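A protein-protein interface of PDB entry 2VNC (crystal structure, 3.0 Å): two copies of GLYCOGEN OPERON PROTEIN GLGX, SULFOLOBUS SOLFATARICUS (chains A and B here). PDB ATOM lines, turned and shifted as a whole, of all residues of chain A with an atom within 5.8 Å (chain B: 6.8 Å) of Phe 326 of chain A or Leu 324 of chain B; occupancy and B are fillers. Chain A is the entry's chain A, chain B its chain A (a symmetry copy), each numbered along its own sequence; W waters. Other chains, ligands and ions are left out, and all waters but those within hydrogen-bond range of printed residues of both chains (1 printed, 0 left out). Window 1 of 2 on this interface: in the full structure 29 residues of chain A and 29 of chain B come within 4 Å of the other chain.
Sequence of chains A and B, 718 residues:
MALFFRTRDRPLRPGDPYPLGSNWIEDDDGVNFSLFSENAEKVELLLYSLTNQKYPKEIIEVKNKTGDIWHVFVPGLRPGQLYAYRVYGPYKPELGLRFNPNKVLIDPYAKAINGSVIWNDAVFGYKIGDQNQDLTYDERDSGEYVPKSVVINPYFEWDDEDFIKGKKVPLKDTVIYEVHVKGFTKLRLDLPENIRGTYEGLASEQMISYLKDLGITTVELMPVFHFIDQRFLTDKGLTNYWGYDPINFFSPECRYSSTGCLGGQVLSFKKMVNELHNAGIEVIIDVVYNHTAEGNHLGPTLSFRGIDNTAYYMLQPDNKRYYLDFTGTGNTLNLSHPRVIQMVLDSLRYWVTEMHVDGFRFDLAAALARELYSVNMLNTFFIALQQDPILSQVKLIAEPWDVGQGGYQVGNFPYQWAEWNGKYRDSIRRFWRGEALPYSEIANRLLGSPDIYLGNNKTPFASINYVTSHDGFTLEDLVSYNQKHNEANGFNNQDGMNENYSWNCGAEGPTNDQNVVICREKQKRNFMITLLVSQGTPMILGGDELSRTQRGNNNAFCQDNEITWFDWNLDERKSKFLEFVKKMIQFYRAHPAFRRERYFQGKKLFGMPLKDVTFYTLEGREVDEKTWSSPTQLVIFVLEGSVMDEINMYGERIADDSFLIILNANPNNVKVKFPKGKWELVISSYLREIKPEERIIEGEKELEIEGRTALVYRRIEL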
ATOM      1  N   MET A 314     -11.793  -6.659   2.249  1.00  0.00           N
ATOM      2  CA  MET A 314     -12.037  -5.461   3.039  1.00  0.00           C
ATOM      3  C   MET A 314     -13.369  -5.533   3.765  1.00  0.00           C
ATOM      4  O   MET A 314     -14.433  -5.497   3.153  1.00  0.00           O
ATOM      5  CB  MET A 314     -11.954  -4.209   2.177  1.00  0.00           C
ATOM      6  CG  MET A 314     -10.536  -3.875   1.821  1.00  0.00           C
ATOM      7  SD  MET A 314     -10.314  -2.162   1.361  1.00  0.00           S
ATOM      8  CE  MET A 314      -8.906  -2.285   0.246  1.00  0.00           C
ATOM      9  N   LEU A 324     -16.782  -4.208   2.382  1.00  0.00           N
ATOM     10  CA  LEU A 324     -16.665  -2.884   1.740  1.00  0.00           C
ATOM     11  C   LEU A 324     -16.753  -3.000   0.226  1.00  0.00           C
ATOM     12  O   LEU A 324     -16.198  -3.919  -0.383  1.00  0.00           O
ATOM     13  CB  LEU A 324     -15.364  -2.176   2.123  1.00  0.00           C
ATOM     14  CG  LEU A 324     -15.273  -1.807   3.594  1.00  0.00           C
ATOM     15  CD1 LEU A 324     -13.858  -1.367   3.949  1.00  0.00           C
ATOM     16  CD2 LEU A 324     -16.303  -0.729   3.931  1.00  0.00           C
ATOM     17  N   ASP A 325     -17.459  -2.046  -0.365  1.00  0.00           N
ATOM     18  CA  ASP A 325     -17.706  -2.018  -1.782  1.00  0.00           C
ATOM     19  C   ASP A 325     -17.289  -0.638  -2.261  1.00  0.00           C
ATOM     20  O   ASP A 325     -17.837   0.348  -1.788  1.00  0.00           O
ATOM     21  CB  ASP A 325     -19.203  -2.225  -2.012  1.00  0.00           C
ATOM     22  CG  ASP A 325     -19.539  -2.661  -3.424  1.00  0.00           C
ATOM     23  OD1 ASP A 325     -18.720  -2.507  -4.356  1.00  0.00           O
ATOM     24  OD2 ASP A 325     -20.654  -3.174  -3.617  1.00  0.00           O
ATOM     25  N   PHE A 326     -16.306  -0.552  -3.158  1.00  0.00           N
ATOM     26  CA  PHE A 326     -16.003   0.721  -3.827  1.00  0.00           C
ATOM     27  C   PHE A 326     -16.580   0.769  -5.239  1.00  0.00           C
ATOM     28  O   PHE A 326     -16.735   1.837  -5.816  1.00  0.00           O
ATOM     29  CB  PHE A 326     -14.499   0.989  -3.865  1.00  0.00           C
ATOM     30  CG  PHE A 326     -13.889   1.212  -2.513  1.00  0.00           C
ATOM     31  CD1 PHE A 326     -13.598   0.141  -1.677  1.00  0.00           C
ATOM     32  CD2 PHE A 326     -13.608   2.499  -2.070  1.00  0.00           C
ATOM     33  CE1 PHE A 326     -13.038   0.348  -0.413  1.00  0.00           C
ATOM     34  CE2 PHE A 326     -13.050   2.715  -0.813  1.00  0.00           C
ATOM     35  CZ  PHE A 326     -12.763   1.635   0.013  1.00  0.00           C
ATOM     36  N   THR A 327     -16.907  -0.396  -5.784  1.00  0.00           N
ATOM     37  CA  THR A 327     -17.317  -0.528  -7.196  1.00  0.00           C
ATOM     38  C   THR A 327     -18.793  -0.775  -7.407  1.00  0.00           C
ATOM     39  O   THR A 327     -19.273  -0.661  -8.530  1.00  0.00           O
ATOM     40  CB  THR A 327     -16.658  -1.722  -7.841  1.00  0.00           C
ATOM     41  OG1 THR A 327     -16.903  -2.870  -7.012  1.00  0.00           O
ATOM     42  CG2 THR A 327     -15.186  -1.478  -7.982  1.00  0.00           C
ATOM     43  N   GLY A 328     -19.498  -1.155  -6.346  1.00  0.00           N
ATOM     44  CA  GLY A 328     -20.906  -1.510  -6.458  1.00  0.00           C
ATOM     45  C   GLY A 328     -21.072  -2.984  -6.780  1.00  0.00           C
ATOM     46  O   GLY A 328     -22.165  -3.440  -7.095  1.00  0.00           O
ATOM     47  N   ASN A 331     -17.546  -6.603  -3.298  1.00  0.00           N
ATOM     48  CA  ASN A 331     -16.318  -6.761  -2.520  1.00  0.00           C
ATOM     49  C   ASN A 331     -15.133  -5.918  -2.949  1.00  0.00           C
ATOM     50  O   ASN A 331     -15.189  -5.214  -3.944  1.00  0.00           O
ATOM     51  CB  ASN A 331     -15.936  -8.239  -2.335  1.00  0.00           C
ATOM     52  CG  ASN A 331     -15.631  -8.940  -3.631  1.00  0.00           C
ATOM     53  OD1 ASN A 331     -15.224  -8.328  -4.599  1.00  0.00           O
ATOM     54  ND2 ASN A 331     -15.806 -10.238  -3.644  1.00  0.00           N
ATOM     55  N   THR A 332     -14.082  -5.979  -2.143  1.00  0.00           N
ATOM     56  CA  THR A 332     -12.817  -5.319  -2.419  1.00  0.00           C
ATOM     57  C   THR A 332     -11.751  -6.199  -1.825  1.00  0.00           C
ATOM     58  O   THR A 332     -11.899  -6.675  -0.685  1.00  0.00           O
ATOM     59  CB  THR A 332     -12.718  -3.931  -1.731  1.00  0.00           C
ATOM     60  OG1 THR A 332     -13.822  -3.114  -2.126  1.00  0.00           O
ATOM     61  CG2 THR A 332     -11.449  -3.226  -2.133  1.00  0.00           C
ATOM     62  N   ALA A 367     -11.774   3.304  -9.360  1.00  0.00           N
ATOM     63  CA  ALA A 367     -12.180   2.510  -8.220  1.00  0.00           C
ATOM     64  C   ALA A 367     -10.957   1.805  -7.637  1.00  0.00           C
ATOM     65  O   ALA A 367     -10.755   1.775  -6.408  1.00  0.00           O
ATOM     66  CB  ALA A 367     -13.234   1.491  -8.642  1.00  0.00           C
ATOM     67  N   ARG A 370      -8.980   4.237  -5.804  1.00  0.00           N
ATOM     68  CA  ARG A 370      -9.694   4.497  -4.554  1.00  0.00           C
ATOM     69  C   ARG A 370      -9.474   3.398  -3.503  1.00  0.00           C
ATOM     70  O   ARG A 370      -9.276   3.710  -2.310  1.00  0.00           O
ATOM     71  CB  ARG A 370     -11.205   4.694  -4.780  1.00  0.00           C
ATOM     72  CG  ARG A 370     -11.975   5.179  -3.528  1.00  0.00           C
ATOM     73  CD  ARG A 370     -11.457   6.539  -3.095  1.00  0.00           C
ATOM     74  NE  ARG A 370     -12.050   7.034  -1.861  1.00  0.00           N
ATOM     75  CZ  ARG A 370     -11.616   6.752  -0.634  1.00  0.00           C
ATOM     76  NH1 ARG A 370     -12.243   7.269   0.401  1.00  0.00           N
ATOM     77  NH2 ARG A 370     -10.569   5.953  -0.433  1.00  0.00           N
ATOM     78  N   GLU A 371      -9.531   2.132  -3.936  1.00  0.00           N
ATOM     79  CA  GLU A 371      -9.350   1.013  -3.021  1.00  0.00           C
ATOM     80  C   GLU A 371      -7.923   1.027  -2.480  1.00  0.00           C
ATOM     81  O   GLU A 371      -7.695   0.936  -1.276  1.00  0.00           O
ATOM     82  CB  GLU A 371      -9.662  -0.315  -3.705  1.00  0.00           C
ATOM     83  CG  GLU A 371     -11.080  -0.389  -4.313  1.00  0.00           C
ATOM     84  CD  GLU A 371     -11.379  -1.685  -5.118  1.00  0.00           C
ATOM     85  OE1 GLU A 371     -10.467  -2.519  -5.347  1.00  0.00           O
ATOM     86  OE2 GLU A 371     -12.555  -1.857  -5.522  1.00  0.00           O
ATOM     87  N   SER A 374      -7.491   3.843  -0.057  1.00  0.00           N
ATOM     88  CA  SER A 374      -8.204   3.401   1.131  1.00  0.00           C
ATOM     89  C   SER A 374      -7.325   2.792   2.241  1.00  0.00           C
ATOM     90  O   SER A 374      -7.649   2.887   3.426  1.00  0.00           O
ATOM     91  CB  SER A 374      -9.236   2.376   0.681  1.00  0.00           C
ATOM     92  OG  SER A 374      -9.746   1.663   1.790  1.00  0.00           O
ATOM     93  N   TYR B 313     -19.596  14.370   1.006  1.00  0.00           N
ATOM     94  CA  TYR B 313     -19.758  12.903   0.877  1.00  0.00           C
ATOM     95  C   TYR B 313     -18.680  12.101   0.147  1.00  0.00           C
ATOM     96  O   TYR B 313     -18.128  12.531  -0.866  1.00  0.00           O
ATOM     97  CB  TYR B 313     -21.142  12.554   0.343  1.00  0.00           C
ATOM     98  CG  TYR B 313     -22.209  12.860   1.353  1.00  0.00           C
ATOM     99  CD1 TYR B 313     -23.194  13.812   1.094  1.00  0.00           C
ATOM    100  CD2 TYR B 313     -22.189  12.240   2.596  1.00  0.00           C
ATOM    101  CE1 TYR B 313     -24.156  14.110   2.052  1.00  0.00           C
ATOM    102  CE2 TYR B 313     -23.135  12.528   3.557  1.00  0.00           C
ATOM    103  CZ  TYR B 313     -24.120  13.458   3.288  1.00  0.00           C
ATOM    104  OH  TYR B 313     -25.059  13.717   4.264  1.00  0.00           O
ATOM    105  N   MET B 314     -18.393  10.919   0.685  1.00  0.00           N
ATOM    106  CA  MET B 314     -17.547   9.955  -0.004  1.00  0.00           C
ATOM    107  C   MET B 314     -18.315   9.208  -1.080  1.00  0.00           C
ATOM    108  O   MET B 314     -19.205   8.411  -0.792  1.00  0.00           O
ATOM    109  CB  MET B 314     -16.905   8.987   0.978  1.00  0.00           C
ATOM    110  CG  MET B 314     -15.798   9.638   1.754  1.00  0.00           C
ATOM    111  SD  MET B 314     -14.640   8.464   2.444  1.00  0.00           S
ATOM    112  CE  MET B 314     -14.058   9.364   3.890  1.00  0.00           C
ATOM    113  N   LEU B 315     -17.965   9.489  -2.326  1.00  0.00           N
ATOM    114  CA  LEU B 315     -18.658   8.886  -3.459  1.00  0.00           C
ATOM    115  C   LEU B 315     -17.888   7.741  -4.101  1.00  0.00           C
ATOM    116  O   LEU B 315     -16.648   7.684  -4.023  1.00  0.00           O
ATOM    117  CB  LEU B 315     -18.981   9.945  -4.504  1.00  0.00           C
ATOM    118  CG  LEU B 315     -20.316  10.668  -4.373  1.00  0.00           C
ATOM    119  CD1 LEU B 315     -20.670  11.005  -2.932  1.00  0.00           C
ATOM    120  CD2 LEU B 315     -20.267  11.908  -5.222  1.00  0.00           C
ATOM    121  N   GLN B 316     -18.639   6.832  -4.718  1.00  0.00           N
ATOM    122  CA  GLN B 316     -18.079   5.724  -5.459  1.00  0.00           C
ATOM    123  C   GLN B 316     -17.458   6.269  -6.705  1.00  0.00           C
ATOM    124  O   GLN B 316     -18.171   6.825  -7.534  1.00  0.00           O
ATOM    125  CB  GLN B 316     -19.177   4.778  -5.873  1.00  0.00           C
ATOM    126  CG  GLN B 316     -19.610   3.851  -4.787  1.00  0.00           C
ATOM    127  CD  GLN B 316     -20.443   2.703  -5.321  1.00  0.00           C
ATOM    128  OE1 GLN B 316     -20.557   2.500  -6.537  1.00  0.00           O
ATOM    129  NE2 GLN B 316     -21.033   1.940  -4.409  1.00  0.00           N
ATOM    130  N   PRO B 317     -16.129   6.110  -6.862  1.00  0.00           N
ATOM    131  CA  PRO B 317     -15.558   6.599  -8.119  1.00  0.00           C
ATOM    132  C   PRO B 317     -16.009   5.637  -9.224  1.00  0.00           C
ATOM    133  O   PRO B 317     -16.245   4.424  -8.949  1.00  0.00           O
ATOM    134  CB  PRO B 317     -14.050   6.550  -7.876  1.00  0.00           C
ATOM    135  CG  PRO B 317     -13.866   5.559  -6.786  1.00  0.00           C
ATOM    136  CD  PRO B 317     -15.125   5.471  -5.994  1.00  0.00           C
ATOM    137  N   ASP B 318     -16.185   6.154 -10.439  1.00  0.00           N
ATOM    138  CA  ASP B 318     -16.749   5.342 -11.533  1.00  0.00           C
ATOM    139  C   ASP B 318     -18.257   5.232 -11.433  1.00  0.00           C
ATOM    140  O   ASP B 318     -18.903   4.799 -12.381  1.00  0.00           O
ATOM    141  CB  ASP B 318     -16.159   3.914 -11.602  1.00  0.00           C
ATOM    142  CG  ASP B 318     -14.686   3.893 -11.975  1.00  0.00           C
ATOM    143  OD1 ASP B 318     -14.287   4.496 -12.997  1.00  0.00           O
ATOM    144  OD2 ASP B 318     -13.925   3.240 -11.237  1.00  0.00           O
ATOM    145  N   ASN B 319     -18.831   5.588 -10.293  1.00  0.00           N
ATOM    146  CA  ASN B 319     -20.278   5.741 -10.243  1.00  0.00           C
ATOM    147  C   ASN B 319     -20.744   6.694  -9.166  1.00  0.00           C
ATOM    148  O   ASN B 319     -21.264   6.276  -8.128  1.00  0.00           O
ATOM    149  CB  ASN B 319     -20.969   4.388 -10.101  1.00  0.00           C
ATOM    150  CG  ASN B 319     -22.413   4.423 -10.571  1.00  0.00           C
ATOM    151  OD1 ASN B 319     -22.937   5.468 -11.008  1.00  0.00           O
ATOM    152  ND2 ASN B 319     -23.068   3.269 -10.487  1.00  0.00           N
ATOM    153  N   TYR B 322     -23.542   6.898  -6.261  1.00  0.00           N
ATOM    154  CA  TYR B 322     -23.548   6.081  -5.044  1.00  0.00           C
ATOM    155  C   TYR B 322     -22.554   6.532  -3.980  1.00  0.00           C
ATOM    156  O   TYR B 322     -21.513   7.127  -4.267  1.00  0.00           O
ATOM    157  CB  TYR B 322     -23.407   4.590  -5.370  1.00  0.00           C
ATOM    158  CG  TYR B 322     -24.474   4.084  -6.331  1.00  0.00           C
ATOM    159  CD1 TYR B 322     -25.825   4.064  -5.962  1.00  0.00           C
ATOM    160  CD2 TYR B 322     -24.137   3.620  -7.599  1.00  0.00           C
ATOM    161  CE1 TYR B 322     -26.811   3.602  -6.834  1.00  0.00           C
ATOM    162  CE2 TYR B 322     -25.114   3.144  -8.470  1.00  0.00           C
ATOM    163  CZ  TYR B 322     -26.448   3.149  -8.081  1.00  0.00           C
ATOM    164  OH  TYR B 322     -27.412   2.701  -8.946  1.00  0.00           O
ATOM    165  N   TYR B 323     -22.921   6.258  -2.739  1.00  0.00           N
ATOM    166  CA  TYR B 323     -22.188   6.732  -1.591  1.00  0.00           C
ATOM    167  C   TYR B 323     -21.432   5.565  -1.028  1.00  0.00           C
ATOM    168  O   TYR B 323     -21.949   4.455  -1.022  1.00  0.00           O
ATOM    169  CB  TYR B 323     -23.168   7.267  -0.534  1.00  0.00           C
ATOM    170  CG  TYR B 323     -23.883   8.536  -0.940  1.00  0.00           C
ATOM    171  CD1 TYR B 323     -23.466   9.780  -0.469  1.00  0.00           C
ATOM    172  CD2 TYR B 323     -24.964   8.492  -1.810  1.00  0.00           C
ATOM    173  CE1 TYR B 323     -24.115  10.944  -0.857  1.00  0.00           C
ATOM    174  CE2 TYR B 323     -25.620   9.649  -2.209  1.00  0.00           C
ATOM    175  CZ  TYR B 323     -25.192  10.866  -1.732  1.00  0.00           C
ATOM    176  OH  TYR B 323     -25.859  11.996  -2.136  1.00  0.00           O
ATOM    177  N   LEU B 324     -20.202   5.815  -0.579  1.00  0.00           N
ATOM    178  CA  LEU B 324     -19.426   4.839   0.212  1.00  0.00           C
ATOM    179  C   LEU B 324     -19.990   4.701   1.618  1.00  0.00           C
ATOM    180  O   LEU B 324     -20.384   5.682   2.254  1.00  0.00           O
ATOM    181  CB  LEU B 324     -17.944   5.217   0.292  1.00  0.00           C
ATOM    182  CG  LEU B 324     -17.223   5.166  -1.044  1.00  0.00           C
ATOM    183  CD1 LEU B 324     -15.848   5.814  -0.935  1.00  0.00           C
ATOM    184  CD2 LEU B 324     -17.130   3.722  -1.537  1.00  0.00           C
ATOM    185  N   ASP B 325     -20.016   3.461   2.086  1.00  0.00           N
ATOM    186  CA  ASP B 325     -20.569   3.120   3.371  1.00  0.00           C
ATOM    187  C   ASP B 325     -19.501   2.321   4.097  1.00  0.00           C
ATOM    188  O   ASP B 325     -19.096   1.279   3.601  1.00  0.00           O
ATOM    189  CB  ASP B 325     -21.811   2.259   3.145  1.00  0.00           C
ATOM    190  CG  ASP B 325     -22.731   2.205   4.349  1.00  0.00           C
ATOM    191  OD1 ASP B 325     -22.323   2.530   5.484  1.00  0.00           O
ATOM    192  OD2 ASP B 325     -23.900   1.826   4.161  1.00  0.00           O
ATOM    193  N   PHE B 326     -19.015   2.809   5.239  1.00  0.00           N
ATOM    194  CA  PHE B 326     -18.151   1.990   6.102  1.00  0.00           C
ATOM    195  C   PHE B 326     -18.918   1.418   7.290  1.00  0.00           C
ATOM    196  O   PHE B 326     -18.481   0.459   7.914  1.00  0.00           O
ATOM    197  CB  PHE B 326     -16.938   2.783   6.592  1.00  0.00           C
ATOM    198  CG  PHE B 326     -15.985   3.169   5.500  1.00  0.00           C
ATOM    199  CD1 PHE B 326     -16.257   4.249   4.667  1.00  0.00           C
ATOM    200  CD2 PHE B 326     -14.814   2.449   5.298  1.00  0.00           C
ATOM    201  CE1 PHE B 326     -15.374   4.604   3.643  1.00  0.00           C
ATOM    202  CE2 PHE B 326     -13.929   2.796   4.281  1.00  0.00           C
ATOM    203  CZ  PHE B 326     -14.211   3.878   3.456  1.00  0.00           C
ATOM    204  N   THR B 327     -20.070   2.006   7.589  1.00  0.00           N
ATOM    205  CA  THR B 327     -20.840   1.678   8.805  1.00  0.00           C
ATOM    206  C   THR B 327     -22.088   0.861   8.562  1.00  0.00           C
ATOM    207  O   THR B 327     -22.663   0.336   9.510  1.00  0.00           O
ATOM    208  CB  THR B 327     -21.354   2.928   9.474  1.00  0.00           C
ATOM    209  OG1 THR B 327     -22.049   3.709   8.489  1.00  0.00           O
ATOM    210  CG2 THR B 327     -20.209   3.705  10.051  1.00  0.00           C
ATOM    211  N   GLY B 330     -25.158   4.065   5.139  1.00  0.00           N
ATOM    212  CA  GLY B 330     -25.483   4.657   3.865  1.00  0.00           C
ATOM    213  C   GLY B 330     -24.545   5.750   3.419  1.00  0.00           C
ATOM    214  O   GLY B 330     -24.400   5.960   2.211  1.00  0.00           O
ATOM    215  N   ASN B 331     -23.918   6.462   4.356  1.00  0.00           N
ATOM    216  CA  ASN B 331     -22.950   7.476   3.944  1.00  0.00           C
ATOM    217  C   ASN B 331     -21.690   7.587   4.779  1.00  0.00           C
ATOM    218  O   ASN B 331     -21.544   6.919   5.790  1.00  0.00           O
ATOM    219  CB  ASN B 331     -23.610   8.846   3.713  1.00  0.00           C
ATOM    220  CG  ASN B 331     -24.226   9.425   4.956  1.00  0.00           C
ATOM    221  OD1 ASN B 331     -23.813   9.134   6.061  1.00  0.00           O
ATOM    222  ND2 ASN B 331     -25.212  10.271   4.777  1.00  0.00           N
ATOM    223  N   THR B 332     -20.772   8.417   4.301  1.00  0.00           N
ATOM    224  CA  THR B 332     -19.534   8.734   4.993  1.00  0.00           C
ATOM    225  C   THR B 332     -19.208  10.157   4.631  1.00  0.00           C
ATOM    226  O   THR B 332     -19.304  10.537   3.450  1.00  0.00           O
ATOM    227  CB  THR B 332     -18.354   7.846   4.518  1.00  0.00           C
ATOM    228  OG1 THR B 332     -18.692   6.465   4.674  1.00  0.00           O
ATOM    229  CG2 THR B 332     -17.120   8.118   5.337  1.00  0.00           C
ATOM    230  N   LEU B 333     -18.823  10.941   5.633  1.00  0.00           N
ATOM    231  CA  LEU B 333     -18.381  12.303   5.375  1.00  0.00           C
ATOM    232  C   LEU B 333     -17.077  12.275   4.604  1.00  0.00           C
ATOM    233  O   LEU B 333     -16.302  11.332   4.717  1.00  0.00           O
ATOM    234  CB  LEU B 333     -18.228  13.113   6.660  1.00  0.00           C
ATOM    235  CG  LEU B 333     -19.490  13.588   7.381  1.00  0.00           C
ATOM    236  CD1 LEU B 333     -19.200  13.821   8.858  1.00  0.00           C
ATOM    237  CD2 LEU B 333     -20.066  14.839   6.740  1.00  0.00           C
ATOM    238  N   ARG B 370     -11.502   3.810  10.353  1.00  0.00           N
ATOM    239  CA  ARG B 370     -11.473   3.283   8.990  1.00  0.00           C
ATOM    240  C   ARG B 370     -11.751   4.359   7.928  1.00  0.00           C
ATOM    241  O   ARG B 370     -11.070   4.390   6.882  1.00  0.00           O
ATOM    242  CB  ARG B 370     -12.457   2.112   8.801  1.00  0.00           C
ATOM    243  CG  ARG B 370     -12.318   1.381   7.443  1.00  0.00           C
ATOM    244  CD  ARG B 370     -10.935   0.762   7.326  1.00  0.00           C
ATOM    245  NE  ARG B 370     -10.674   0.139   6.037  1.00  0.00           N
ATOM    246  CZ  ARG B 370     -10.212   0.770   4.959  1.00  0.00           C
ATOM    247  NH1 ARG B 370     -10.014   0.086   3.853  1.00  0.00           N
ATOM    248  NH2 ARG B 370      -9.956   2.078   4.975  1.00  0.00           N
ATOM    249  N   GLU B 371     -12.750   5.213   8.186  1.00  0.00           N
ATOM    250  CA  GLU B 371     -13.107   6.263   7.241  1.00  0.00           C
ATOM    251  C   GLU B 371     -11.952   7.256   7.129  1.00  0.00           C
ATOM    252  O   GLU B 371     -11.515   7.608   6.036  1.00  0.00           O
ATOM    253  CB  GLU B 371     -14.395   6.967   7.660  1.00  0.00           C
ATOM    254  CG  GLU B 371     -15.601   6.017   7.831  1.00  0.00           C
ATOM    255  CD  GLU B 371     -16.892   6.692   8.371  1.00  0.00           C
ATOM    256  OE1 GLU B 371     -16.875   7.889   8.755  1.00  0.00           O
ATOM    257  OE2 GLU B 371     -17.937   5.997   8.406  1.00  0.00           O
ATOM    258  N   SER B 374      -9.107   5.720   5.252  1.00  0.00           N
ATOM    259  CA  SER B 374      -9.560   5.707   3.870  1.00  0.00           C
ATOM    260  C   SER B 374      -9.038   6.862   2.993  1.00  0.00           C
ATOM    261  O   SER B 374      -8.866   6.708   1.782  1.00  0.00           O
ATOM    262  CB  SER B 374     -11.081   5.735   3.895  1.00  0.00           C
ATOM    263  OG  SER B 374     -11.596   6.049   2.616  1.00  0.00           O
HETATM  264  O   HOH W   1     -14.129   8.512  -2.664  1.00  0.00           O
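OD2 of Asp 318 of chain B is in hydrogen-bond range of N of Ala 367 of chain A (2.9 Å). The guanidinium group of Arg 370 of chain A is in hydrogen-bond range of the side-chain sulfur of Met 314 of chain B. The side-chain hydroxyl (OG) of Ser 374 of chain A sits at hydrogen-bond distance from the guanidinium group (NH1) of Arg 370 of chain B. The guanidinium group of Arg 370 of chain A is in hydrogen-bond range of the side-chain hydroxyl of Ser 374 of chain B (2.6 Å). SD of Met 314 of chain A sits at hydrogen-bond distance from NH1 of Arg 370 of chain B (3.4 Å).
The backbone NH of Gly 328 of chain A is in hydrogen-bond range of the side-chain carboxylate of Asp 325 of chain A (2.5 Å). The backbone NH of Met 314 of chain B is in hydrogen-bond range of the backbone carbonyl oxygen of Thr 332 of chain B, 2.9 Å away. The side-chain carboxylate of Asp 325 of chain B is in hydrogen-bond range of the backbone NH of Thr 327 of chain B, 3.1 Å away. The side-chain carboxylate (OD2) of Asp 325 of chain B lies within hydrogen-bond range of the backbone NH (N) of Gly 330 of chain B (2.7 Å). OD1 of Asp 325 of chain A is in hydrogen-bond range of N of Thr 327 of chain A. N of Gln 316 of chain B is in hydrogen-bond range of O of Tyr 322 of chain B (2.9 Å).
Among the printed residues, merely in contact across the chains: Leu 324 of chain A with Asp 325 of chain B (3.5 Å), Leu 324 of chain A with Phe 326 of chain B (3.8 Å), Asp 325 of chain A with Leu 324 of chain B (3.5 Å), Phe 326 of chain A with Gln 316 of chain B (3.7 Å), Phe 326 of chain A with Pro 317 of chain B (3.98 Å), Phe 326 of chain A with Leu 324 of chain B (3.8 Å), Thr 327 of chain A with Gln 316 of chain B (3.8 Å), Gly 328 of chain A with Gln 316 of chain B (3.8 Å), Ala 367 of chain A with Pro 317 of chain B (3.8 Å), Arg 370 of chain A with Pro 317 of chain B (3.4 Å) and Ser 374 of chain A with Ser 374 of chain B (3.4 Å).
Printed residues of chain B within 4 Å of Leu 324 of chain A: Asp 325 and Phe 326. Printed residues of chain B within 4 Å of Asp 325 of chain A: Leu 324 (3.5 Å). Phe 326 of chain A touches three residues of chain B. Tyr 323 of chain B touches none of the printed residues of chain A. Leu 324 of chain B touches two residues of chain A. Thr 327 of chain B touches none of the printed residues of chain A. The nearest residue of chain B that does not touch Phe 326 of chain A is Phe 326 of chain B (4.4 Å). The nearest printed residue of chain A that does not touch Phe 326 of chain B is Phe 326 of chain A (4.4 Å).
Of the 20 printed residues of chain B, 9 touch a printed residue of chain A. Printed residues of chain B that touch a printed residue of chain A: Met 314, Gln 316, Pro 317, Asp 318, Leu 324, Asp 325, Phe 326, Arg 370 and Ser 374. Hydrophobic or aromatic side chains of chain B that line the printed part of chain A: Met 314, Pro 317, Leu 324 and Phe 326. Among the printed residues, no Asp or Glu carboxylate lies within 4 Å of a Lys or Arg side-chain nitrogen of the other chain.
Met 314 of chain A touches Arg 370 of chain B, and with the chains exchanged Arg 370 of chain A touches Met 314 of chain B. Leu 324 of chain A touches Asp 325 of chain B, and with the chains exchanged Asp 325 of chain A touches Leu 324 of chain B. Leu 324 of chain A touches Phe 326 of chain B, and with the chains exchanged Phe 326 of chain A touches Leu 324 of chain B. Ser 374 of chain B touches its own counterpart, Ser 374 of chain A. Positions printed for both chains: 314, 324, 325, 326, 327, 331, 332, 370, 371 and 374.
Water W1 bridges the guanidinium group (NE) of Arg 370 of chain A (2.7 Å) and the backbone carbonyl oxygen (O) of Leu 315 of chain B (3.0 Å).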
